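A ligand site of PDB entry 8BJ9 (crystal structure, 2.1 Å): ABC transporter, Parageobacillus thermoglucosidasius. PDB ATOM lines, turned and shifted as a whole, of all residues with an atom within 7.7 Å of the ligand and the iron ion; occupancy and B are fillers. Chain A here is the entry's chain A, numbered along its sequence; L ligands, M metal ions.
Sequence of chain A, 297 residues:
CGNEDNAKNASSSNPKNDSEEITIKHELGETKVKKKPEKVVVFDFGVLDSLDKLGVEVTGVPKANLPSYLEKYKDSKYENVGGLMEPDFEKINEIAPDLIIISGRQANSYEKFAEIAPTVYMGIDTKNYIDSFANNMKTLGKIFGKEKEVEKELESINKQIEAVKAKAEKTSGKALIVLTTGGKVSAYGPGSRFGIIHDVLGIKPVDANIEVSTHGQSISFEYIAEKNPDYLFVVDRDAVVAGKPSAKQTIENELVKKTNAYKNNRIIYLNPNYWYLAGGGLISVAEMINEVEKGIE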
ATOM      1  N   PHE A  45      21.240  -7.330   2.336  1.00  0.00           N
ATOM      2  CA  PHE A  45      20.378  -8.324   2.959  1.00  0.00           C
ATOM      3  C   PHE A  45      19.111  -7.705   3.556  1.00  0.00           C
ATOM      4  O   PHE A  45      18.061  -8.336   3.559  1.00  0.00           O
ATOM      5  CB  PHE A  45      21.195  -9.159   3.943  1.00  0.00           C
ATOM      6  CG  PHE A  45      22.138 -10.140   3.290  1.00  0.00           C
ATOM      7  CD1 PHE A  45      21.708 -10.925   2.221  1.00  0.00           C
ATOM      8  CD2 PHE A  45      23.438 -10.295   3.746  1.00  0.00           C
ATOM      9  CE1 PHE A  45      22.566 -11.848   1.631  1.00  0.00           C
ATOM     10  CE2 PHE A  45      24.291 -11.221   3.137  1.00  0.00           C
ATOM     11  CZ  PHE A  45      23.845 -12.002   2.094  1.00  0.00           C
ATOM     12  N   ASN A  65      27.272 -15.377   2.546  1.00  0.00           N
ATOM     13  CA  ASN A  65      27.097 -14.593   3.752  1.00  0.00           C
ATOM     14  C   ASN A  65      25.622 -14.546   4.165  1.00  0.00           C
ATOM     15  O   ASN A  65      25.239 -13.689   4.963  1.00  0.00           O
ATOM     16  CB  ASN A  65      27.588 -13.162   3.536  1.00  0.00           C
ATOM     17  CG  ASN A  65      29.073 -13.140   3.226  1.00  0.00           C
ATOM     18  OD1 ASN A  65      29.466 -12.748   2.131  1.00  0.00           O
ATOM     19  ND2 ASN A  65      29.886 -13.577   4.174  1.00  0.00           N
ATOM     20  N   GLY A  83      29.821 -13.678  -2.638  1.00  0.00           N
ATOM     21  CA  GLY A  83      29.811 -13.117  -1.295  1.00  0.00           C
ATOM     22  C   GLY A  83      29.622 -11.602  -1.339  1.00  0.00           C
ATOM     23  O   GLY A  83      29.797 -10.960  -2.385  1.00  0.00           O
ATOM     24  N   LEU A  84      29.327 -11.041  -0.164  1.00  0.00           N
ATOM     25  CA  LEU A  84      29.177  -9.598   0.025  1.00  0.00           C
ATOM     26  C   LEU A  84      30.430  -8.821  -0.424  1.00  0.00           C
ATOM     27  O   LEU A  84      30.320  -7.746  -1.007  1.00  0.00           O
ATOM     28  CB  LEU A  84      28.927  -9.353   1.510  1.00  0.00           C
ATOM     29  CG  LEU A  84      27.537  -9.710   2.029  1.00  0.00           C
ATOM     30  CD1 LEU A  84      27.493  -9.477   3.540  1.00  0.00           C
ATOM     31  CD2 LEU A  84      26.459  -8.881   1.319  1.00  0.00           C
ATOM     32  N   MET A  85      31.614  -9.360  -0.116  1.00  0.00           N
ATOM     33  CA  MET A  85      32.860  -8.676  -0.463  1.00  0.00           C
ATOM     34  C   MET A  85      33.476  -9.271  -1.734  1.00  0.00           C
ATOM     35  O   MET A  85      34.483  -8.754  -2.218  1.00  0.00           O
ATOM     36  CB  MET A  85      33.862  -8.795   0.703  1.00  0.00           C
ATOM     37  CG  MET A  85      33.332  -8.270   2.040  1.00  0.00           C
ATOM     38  SD  MET A  85      32.843  -6.510   2.043  1.00  0.00           S
ATOM     39  CE  MET A  85      32.619  -6.278   3.799  1.00  0.00           C
ATOM     40  N   SER A 103      24.728  -2.106  -1.704  1.00  0.00           N
ATOM     41  CA  SER A 103      24.823  -1.115  -0.634  1.00  0.00           C
ATOM     42  C   SER A 103      26.304  -0.861  -0.325  1.00  0.00           C
ATOM     43  O   SER A 103      27.164  -1.026  -1.201  1.00  0.00           O
ATOM     44  CB  SER A 103      23.998  -1.525   0.572  1.00  0.00           C
ATOM     45  OG  SER A 103      24.431  -2.767   1.111  1.00  0.00           O
ATOM     46  N   GLY A 104      26.576  -0.420   0.905  1.00  0.00           N
ATOM     47  CA  GLY A 104      27.839   0.229   1.232  1.00  0.00           C
ATOM     48  C   GLY A 104      29.042  -0.692   1.066  1.00  0.00           C
ATOM     49  O   GLY A 104      30.112  -0.245   0.624  1.00  0.00           O
ATOM     50  N   ARG A 105      28.865  -1.987   1.366  1.00  0.00           N
ATOM     51  CA  ARG A 105      29.931  -2.963   1.235  1.00  0.00           C
ATOM     52  C   ARG A 105      30.391  -3.087  -0.234  1.00  0.00           C
ATOM     53  O   ARG A 105      31.483  -3.595  -0.476  1.00  0.00           O
ATOM     54  CB  ARG A 105      29.484  -4.334   1.737  1.00  0.00           C
ATOM     55  CG  ARG A 105      29.161  -4.399   3.230  1.00  0.00           C
ATOM     56  CD  ARG A 105      29.223  -5.839   3.735  1.00  0.00           C
ATOM     57  NE  ARG A 105      29.169  -6.009   5.182  1.00  0.00           N
ATOM     58  CZ  ARG A 105      28.049  -5.976   5.912  1.00  0.00           C
ATOM     59  NH1 ARG A 105      28.052  -6.293   7.189  1.00  0.00           N
ATOM     60  NH2 ARG A 105      26.916  -5.640   5.327  1.00  0.00           N
ATOM     61  N   GLN A 106      29.565  -2.667  -1.207  1.00  0.00           N
ATOM     62  CA  GLN A 106      29.908  -2.792  -2.614  1.00  0.00           C
ATOM     63  C   GLN A 106      30.056  -1.427  -3.299  1.00  0.00           C
ATOM     64  O   GLN A 106      30.386  -1.363  -4.494  1.00  0.00           O
ATOM     65  CB  GLN A 106      28.858  -3.654  -3.326  1.00  0.00           C
ATOM     66  CG  GLN A 106      28.676  -5.046  -2.699  1.00  0.00           C
ATOM     67  CD  GLN A 106      27.600  -5.140  -1.645  1.00  0.00           C
ATOM     68  OE1 GLN A 106      26.701  -4.295  -1.574  1.00  0.00           O
ATOM     69  NE2 GLN A 106      27.651  -6.213  -0.859  1.00  0.00           N
ATOM     70  N   ALA A 107      29.848  -0.332  -2.545  1.00  0.00           N
ATOM     71  CA  ALA A 107      29.907   1.023  -3.112  1.00  0.00           C
ATOM     72  C   ALA A 107      31.041   1.133  -4.125  1.00  0.00           C
ATOM     73  O   ALA A 107      30.806   1.614  -5.228  1.00  0.00           O
ATOM     74  CB  ALA A 107      30.082   2.062  -2.024  1.00  0.00           C
ATOM     75  N   ASN A 108      32.247   0.680  -3.752  1.00  0.00           N
ATOM     76  CA  ASN A 108      33.425   0.853  -4.587  1.00  0.00           C
ATOM     77  C   ASN A 108      33.338   0.046  -5.880  1.00  0.00           C
ATOM     78  O   ASN A 108      34.068   0.341  -6.822  1.00  0.00           O
ATOM     79  CB  ASN A 108      34.721   0.537  -3.848  1.00  0.00           C
ATOM     80  CG  ASN A 108      35.217   1.700  -3.009  1.00  0.00           C
ATOM     81  OD1 ASN A 108      35.149   2.858  -3.427  1.00  0.00           O
ATOM     82  ND2 ASN A 108      35.699   1.400  -1.816  1.00  0.00           N
ATOM     83  N   TYR A 121      22.051   1.927  -5.953  1.00  0.00           N
ATOM     84  CA  TYR A 121      22.712   1.865  -4.656  1.00  0.00           C
ATOM     85  C   TYR A 121      21.731   2.269  -3.570  1.00  0.00           C
ATOM     86  O   TYR A 121      21.059   3.280  -3.701  1.00  0.00           O
ATOM     87  CB  TYR A 121      23.958   2.754  -4.659  1.00  0.00           C
ATOM     88  CG  TYR A 121      24.590   2.878  -3.304  1.00  0.00           C
ATOM     89  CD1 TYR A 121      25.528   1.965  -2.853  1.00  0.00           C
ATOM     90  CD2 TYR A 121      24.190   3.881  -2.437  1.00  0.00           C
ATOM     91  CE1 TYR A 121      26.098   2.082  -1.594  1.00  0.00           C
ATOM     92  CE2 TYR A 121      24.747   4.003  -1.174  1.00  0.00           C
ATOM     93  CZ  TYR A 121      25.708   3.113  -0.756  1.00  0.00           C
ATOM     94  OH  TYR A 121      26.255   3.242   0.488  1.00  0.00           O
ATOM     95  N   LEU A 179      31.072  -3.886  19.767  1.00  0.00           N
ATOM     96  CA  LEU A 179      31.214  -4.955  18.776  1.00  0.00           C
ATOM     97  C   LEU A 179      32.474  -5.746  19.117  1.00  0.00           C
ATOM     98  O   LEU A 179      33.516  -5.158  19.413  1.00  0.00           O
ATOM     99  CB  LEU A 179      31.321  -4.329  17.381  1.00  0.00           C
ATOM    100  CG  LEU A 179      31.530  -5.284  16.200  1.00  0.00           C
ATOM    101  CD1 LEU A 179      30.354  -5.240  15.236  1.00  0.00           C
ATOM    102  CD2 LEU A 179      32.832  -4.977  15.473  1.00  0.00           C
ATOM    103  N   TYR A 188      30.224   1.961  19.293  1.00  0.00           N
ATOM    104  CA  TYR A 188      29.358   2.770  18.447  1.00  0.00           C
ATOM    105  C   TYR A 188      28.475   3.643  19.342  1.00  0.00           C
ATOM    106  O   TYR A 188      28.044   3.201  20.405  1.00  0.00           O
ATOM    107  CB  TYR A 188      28.481   1.915  17.534  1.00  0.00           C
ATOM    108  CG  TYR A 188      29.222   0.986  16.601  1.00  0.00           C
ATOM    109  CD1 TYR A 188      29.889  -0.122  17.090  1.00  0.00           C
ATOM    110  CD2 TYR A 188      29.247   1.219  15.241  1.00  0.00           C
ATOM    111  CE1 TYR A 188      30.561  -0.986  16.236  1.00  0.00           C
ATOM    112  CE2 TYR A 188      29.908   0.361  14.368  1.00  0.00           C
ATOM    113  CZ  TYR A 188      30.566  -0.740  14.870  1.00  0.00           C
ATOM    114  OH  TYR A 188      31.215  -1.615  14.035  1.00  0.00           O
ATOM    115  N   ARG A 193      26.408   3.101  12.657  1.00  0.00           N
ATOM    116  CA  ARG A 193      25.576   2.097  12.018  1.00  0.00           C
ATOM    117  C   ARG A 193      24.603   1.487  13.039  1.00  0.00           C
ATOM    118  O   ARG A 193      23.603   0.898  12.644  1.00  0.00           O
ATOM    119  CB  ARG A 193      26.426   1.028  11.325  1.00  0.00           C
ATOM    120  CG  ARG A 193      27.142   0.069  12.267  1.00  0.00           C
ATOM    121  CD  ARG A 193      28.235  -0.764  11.602  1.00  0.00           C
ATOM    122  NE  ARG A 193      27.768  -1.790  10.679  1.00  0.00           N
ATOM    123  CZ  ARG A 193      28.590  -2.562   9.950  1.00  0.00           C
ATOM    124  NH1 ARG A 193      29.895  -2.477  10.101  1.00  0.00           N
ATOM    125  NH2 ARG A 193      28.102  -3.433   9.096  1.00  0.00           N
ATOM    126  N   THR A 214      32.924   2.581  10.516  1.00  0.00           N
ATOM    127  CA  THR A 214      32.104   1.470  10.039  1.00  0.00           C
ATOM    128  C   THR A 214      32.390   0.209  10.856  1.00  0.00           C
ATOM    129  O   THR A 214      31.464  -0.577  11.085  1.00  0.00           O
ATOM    130  CB  THR A 214      32.197   1.272   8.516  1.00  0.00           C
ATOM    131  OG1 THR A 214      33.333   0.465   8.208  1.00  0.00           O
ATOM    132  CG2 THR A 214      32.240   2.566   7.729  1.00  0.00           C
ATOM    133  N   HIS A 215      33.634  -0.017  11.321  1.00  0.00           N
ATOM    134  CA  HIS A 215      33.856  -1.143  12.226  1.00  0.00           C
ATOM    135  C   HIS A 215      34.048  -0.688  13.674  1.00  0.00           C
ATOM    136  O   HIS A 215      34.417  -1.500  14.523  1.00  0.00           O
ATOM    137  CB  HIS A 215      34.989  -2.049  11.740  1.00  0.00           C
ATOM    138  CG  HIS A 215      34.501  -2.916  10.640  1.00  0.00           C
ATOM    139  ND1 HIS A 215      34.767  -2.625   9.325  1.00  0.00           N
ATOM    140  CD2 HIS A 215      33.715  -4.007  10.630  1.00  0.00           C
ATOM    141  CE1 HIS A 215      34.207  -3.542   8.557  1.00  0.00           C
ATOM    142  NE2 HIS A 215      33.563  -4.391   9.328  1.00  0.00           N
ATOM    143  N   ARG A 237      30.646  -9.994  16.030  1.00  0.00           N
ATOM    144  CA  ARG A 237      30.962  -9.922  14.613  1.00  0.00           C
ATOM    145  C   ARG A 237      31.438 -11.294  14.150  1.00  0.00           C
ATOM    146  O   ARG A 237      31.021 -11.740  13.078  1.00  0.00           O
ATOM    147  CB  ARG A 237      32.009  -8.857  14.311  1.00  0.00           C
ATOM    148  CG  ARG A 237      32.302  -8.728  12.819  1.00  0.00           C
ATOM    149  CD  ARG A 237      33.269  -7.611  12.473  1.00  0.00           C
ATOM    150  NE  ARG A 237      33.689  -7.711  11.078  1.00  0.00           N
ATOM    151  CZ  ARG A 237      34.884  -8.157  10.673  1.00  0.00           C
ATOM    152  NH1 ARG A 237      35.744  -8.649  11.558  1.00  0.00           N
ATOM    153  NH2 ARG A 237      35.202  -8.141   9.392  1.00  0.00           N
ATOM    154  N   VAL A 240      29.314 -14.080  12.616  1.00  0.00           N
ATOM    155  CA  VAL A 240      28.776 -13.982  11.259  1.00  0.00           C
ATOM    156  C   VAL A 240      29.888 -13.859  10.209  1.00  0.00           C
ATOM    157  O   VAL A 240      29.637 -14.181   9.050  1.00  0.00           O
ATOM    158  CB  VAL A 240      27.727 -12.849  11.103  1.00  0.00           C
ATOM    159  CG1 VAL A 240      26.386 -13.251  11.687  1.00  0.00           C
ATOM    160  CG2 VAL A 240      28.192 -11.520  11.661  1.00  0.00           C
ATOM    161  N   VAL A 241      31.082 -13.399  10.577  1.00  0.00           N
ATOM    162  CA  VAL A 241      32.169 -13.245   9.617  1.00  0.00           C
ATOM    163  C   VAL A 241      33.164 -14.402   9.731  1.00  0.00           C
ATOM    164  O   VAL A 241      33.879 -14.701   8.776  1.00  0.00           O
ATOM    165  CB  VAL A 241      32.851 -11.862   9.769  1.00  0.00           C
ATOM    166  CG1 VAL A 241      34.109 -11.739   8.925  1.00  0.00           C
ATOM    167  CG2 VAL A 241      31.886 -10.731   9.445  1.00  0.00           C
ATOM    168  N   ALA A 242      33.237 -15.061  10.896  1.00  0.00           N
ATOM    169  CA  ALA A 242      34.111 -16.209  11.041  1.00  0.00           C
ATOM    170  C   ALA A 242      33.288 -17.487  11.179  1.00  0.00           C
ATOM    171  O   ALA A 242      33.790 -18.573  10.909  1.00  0.00           O
ATOM    172  CB  ALA A 242      35.019 -15.997  12.221  1.00  0.00           C
ATOM    173  N   TYR A 276      24.423  -6.892  11.965  1.00  0.00           N
ATOM    174  CA  TYR A 276      25.670  -6.644  11.266  1.00  0.00           C
ATOM    175  C   TYR A 276      25.554  -6.997   9.775  1.00  0.00           C
ATOM    176  O   TYR A 276      25.820  -6.149   8.924  1.00  0.00           O
ATOM    177  CB  TYR A 276      26.791  -7.408  11.983  1.00  0.00           C
ATOM    178  CG  TYR A 276      28.147  -7.111  11.399  1.00  0.00           C
ATOM    179  CD1 TYR A 276      28.849  -5.965  11.751  1.00  0.00           C
ATOM    180  CD2 TYR A 276      28.683  -7.937  10.436  1.00  0.00           C
ATOM    181  CE1 TYR A 276      30.085  -5.680  11.179  1.00  0.00           C
ATOM    182  CE2 TYR A 276      29.915  -7.666   9.868  1.00  0.00           C
ATOM    183  CZ  TYR A 276      30.616  -6.531  10.232  1.00  0.00           C
ATOM    184  OH  TYR A 276      31.834  -6.311   9.655  1.00  0.00           O
ATOM    185  N   LEU A 277      25.112  -8.231   9.463  1.00  0.00           N
ATOM    186  CA  LEU A 277      24.981  -8.658   8.075  1.00  0.00           C
ATOM    187  C   LEU A 277      23.803  -7.966   7.367  1.00  0.00           C
ATOM    188  O   LEU A 277      23.858  -7.788   6.154  1.00  0.00           O
ATOM    189  CB  LEU A 277      24.764 -10.187   8.017  1.00  0.00           C
ATOM    190  CG  LEU A 277      25.977 -11.067   8.313  1.00  0.00           C
ATOM    191  CD1 LEU A 277      25.604 -12.526   8.160  1.00  0.00           C
ATOM    192  CD2 LEU A 277      27.150 -10.719   7.411  1.00  0.00           C
HETATM  193  C1  LIG L   1      30.572  -8.923   6.145  1.00  0.00           C
HETATM  194  C2  LIG L   1      31.328  -7.875   6.653  1.00  0.00           C
HETATM  195  C3  LIG L   1      32.719  -7.969   6.662  1.00  0.00           C
HETATM  196  C4  LIG L   1      33.360  -9.118   6.171  1.00  0.00           C
HETATM  197  C5  LIG L   1      32.571 -10.148   5.661  1.00  0.00           C
HETATM  198  C6  LIG L   1      31.209 -10.063   5.654  1.00  0.00           C
HETATM  199  C7  LIG L   1      34.844  -9.223   6.138  1.00  0.00           C
HETATM  200  N1  LIG L   1      35.531  -8.089   6.101  1.00  0.00           N
HETATM  201  O1  LIG L   1      35.376 -10.330   6.053  1.00  0.00           O
HETATM  202  C8  LIG L   1      36.930  -7.996   5.725  1.00  0.00           C
HETATM  203  C9  LIG L   1      37.373  -6.544   5.587  1.00  0.00           C
HETATM  204  C10 LIG L   1      36.225  -5.643   5.158  1.00  0.00           C
HETATM  205  N2  LIG L   1      34.288  -3.527   4.385  1.00  0.00           N
HETATM  206  C11 LIG L   1      33.467  -2.496   4.175  1.00  0.00           C
HETATM  207  C12 LIG L   1      32.170  -2.447   4.900  1.00  0.00           C
HETATM  208  O2  LIG L   1      33.767  -1.556   3.426  1.00  0.00           O
HETATM  209  C13 LIG L   1      31.906  -3.352   5.942  1.00  0.00           C
HETATM  210  C14 LIG L   1      30.701  -3.292   6.644  1.00  0.00           C
HETATM  211  C15 LIG L   1      29.756  -2.329   6.317  1.00  0.00           C
HETATM  212  C16 LIG L   1      30.016  -1.426   5.288  1.00  0.00           C
HETATM  213  C17 LIG L   1      31.198  -1.475   4.603  1.00  0.00           C
HETATM  214  O3  LIG L   1      32.769  -4.343   6.324  1.00  0.00           O
HETATM  215  O4  LIG L   1      30.566  -4.246   7.627  1.00  0.00           O
HETATM  216  C18 LIG L   1      36.633  -4.269   4.680  1.00  0.00           C
HETATM  217  O5  LIG L   1      33.370  -6.861   7.187  1.00  0.00           O
HETATM  218  C19 LIG L   1      35.608  -3.600   3.773  1.00  0.00           C
HETATM  219  O6  LIG L   1      30.783  -6.702   7.118  1.00  0.00           O
HETATM  220 FE    FE M   1      32.138  -5.430   7.864  1.00  0.00          FE
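An oxygen (O6) of the ligand sits close to the guanidinium group (NE) of Arg 105, 2.6 Å away. An oxygen (O4) of the ligand sits close to the guanidinium group of Arg 193, 3.0 Å away. O5 of the ligand lies close to NH2 of Arg 237, at 3.1 Å.
Within 4 Å of the iron ion: His 215 and Tyr 276. The nearest printed residue that does not touch the iron ion is Arg 105 (4.04 Å).
Residues that only touch the ligand: Met 85 and Val 241. Hydrophobic or aromatic side chains that line the ligand: Met 85, His 215, Val 241 and Tyr 276. Of the 23 residues printed, 7 come within 4 Å of the ligand.
The iron ion is bound by an oxygen (O4) of the ligand, at 2.0 Å. The iron ion is bound by O3 of the ligand, at 2.0 Å. An oxygen (O6) of the ligand is bound to the iron ion, at 2.0 Å. An oxygen (O5) of the ligand is bound to the iron ion. The iron ion is bound by OH of Tyr 276, 2.0 Å away. NE2 of His 215 is bound to the iron ion (2.3 Å). The iron ion has six donor atoms within binding distance.
NH1 of Arg 105 lies within hydrogen-bond range of O of Tyr 276. NE of Arg 237 lies close to OH of Tyr 276 (2.7 Å). O of His 215 lies close to OH of Tyr 188, at 3.2 Å. The guanidinium group (NH1) of Arg 193 lies within hydrogen-bond range of the backbone carbonyl oxygen (O) of Thr 214 (2.7 Å).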
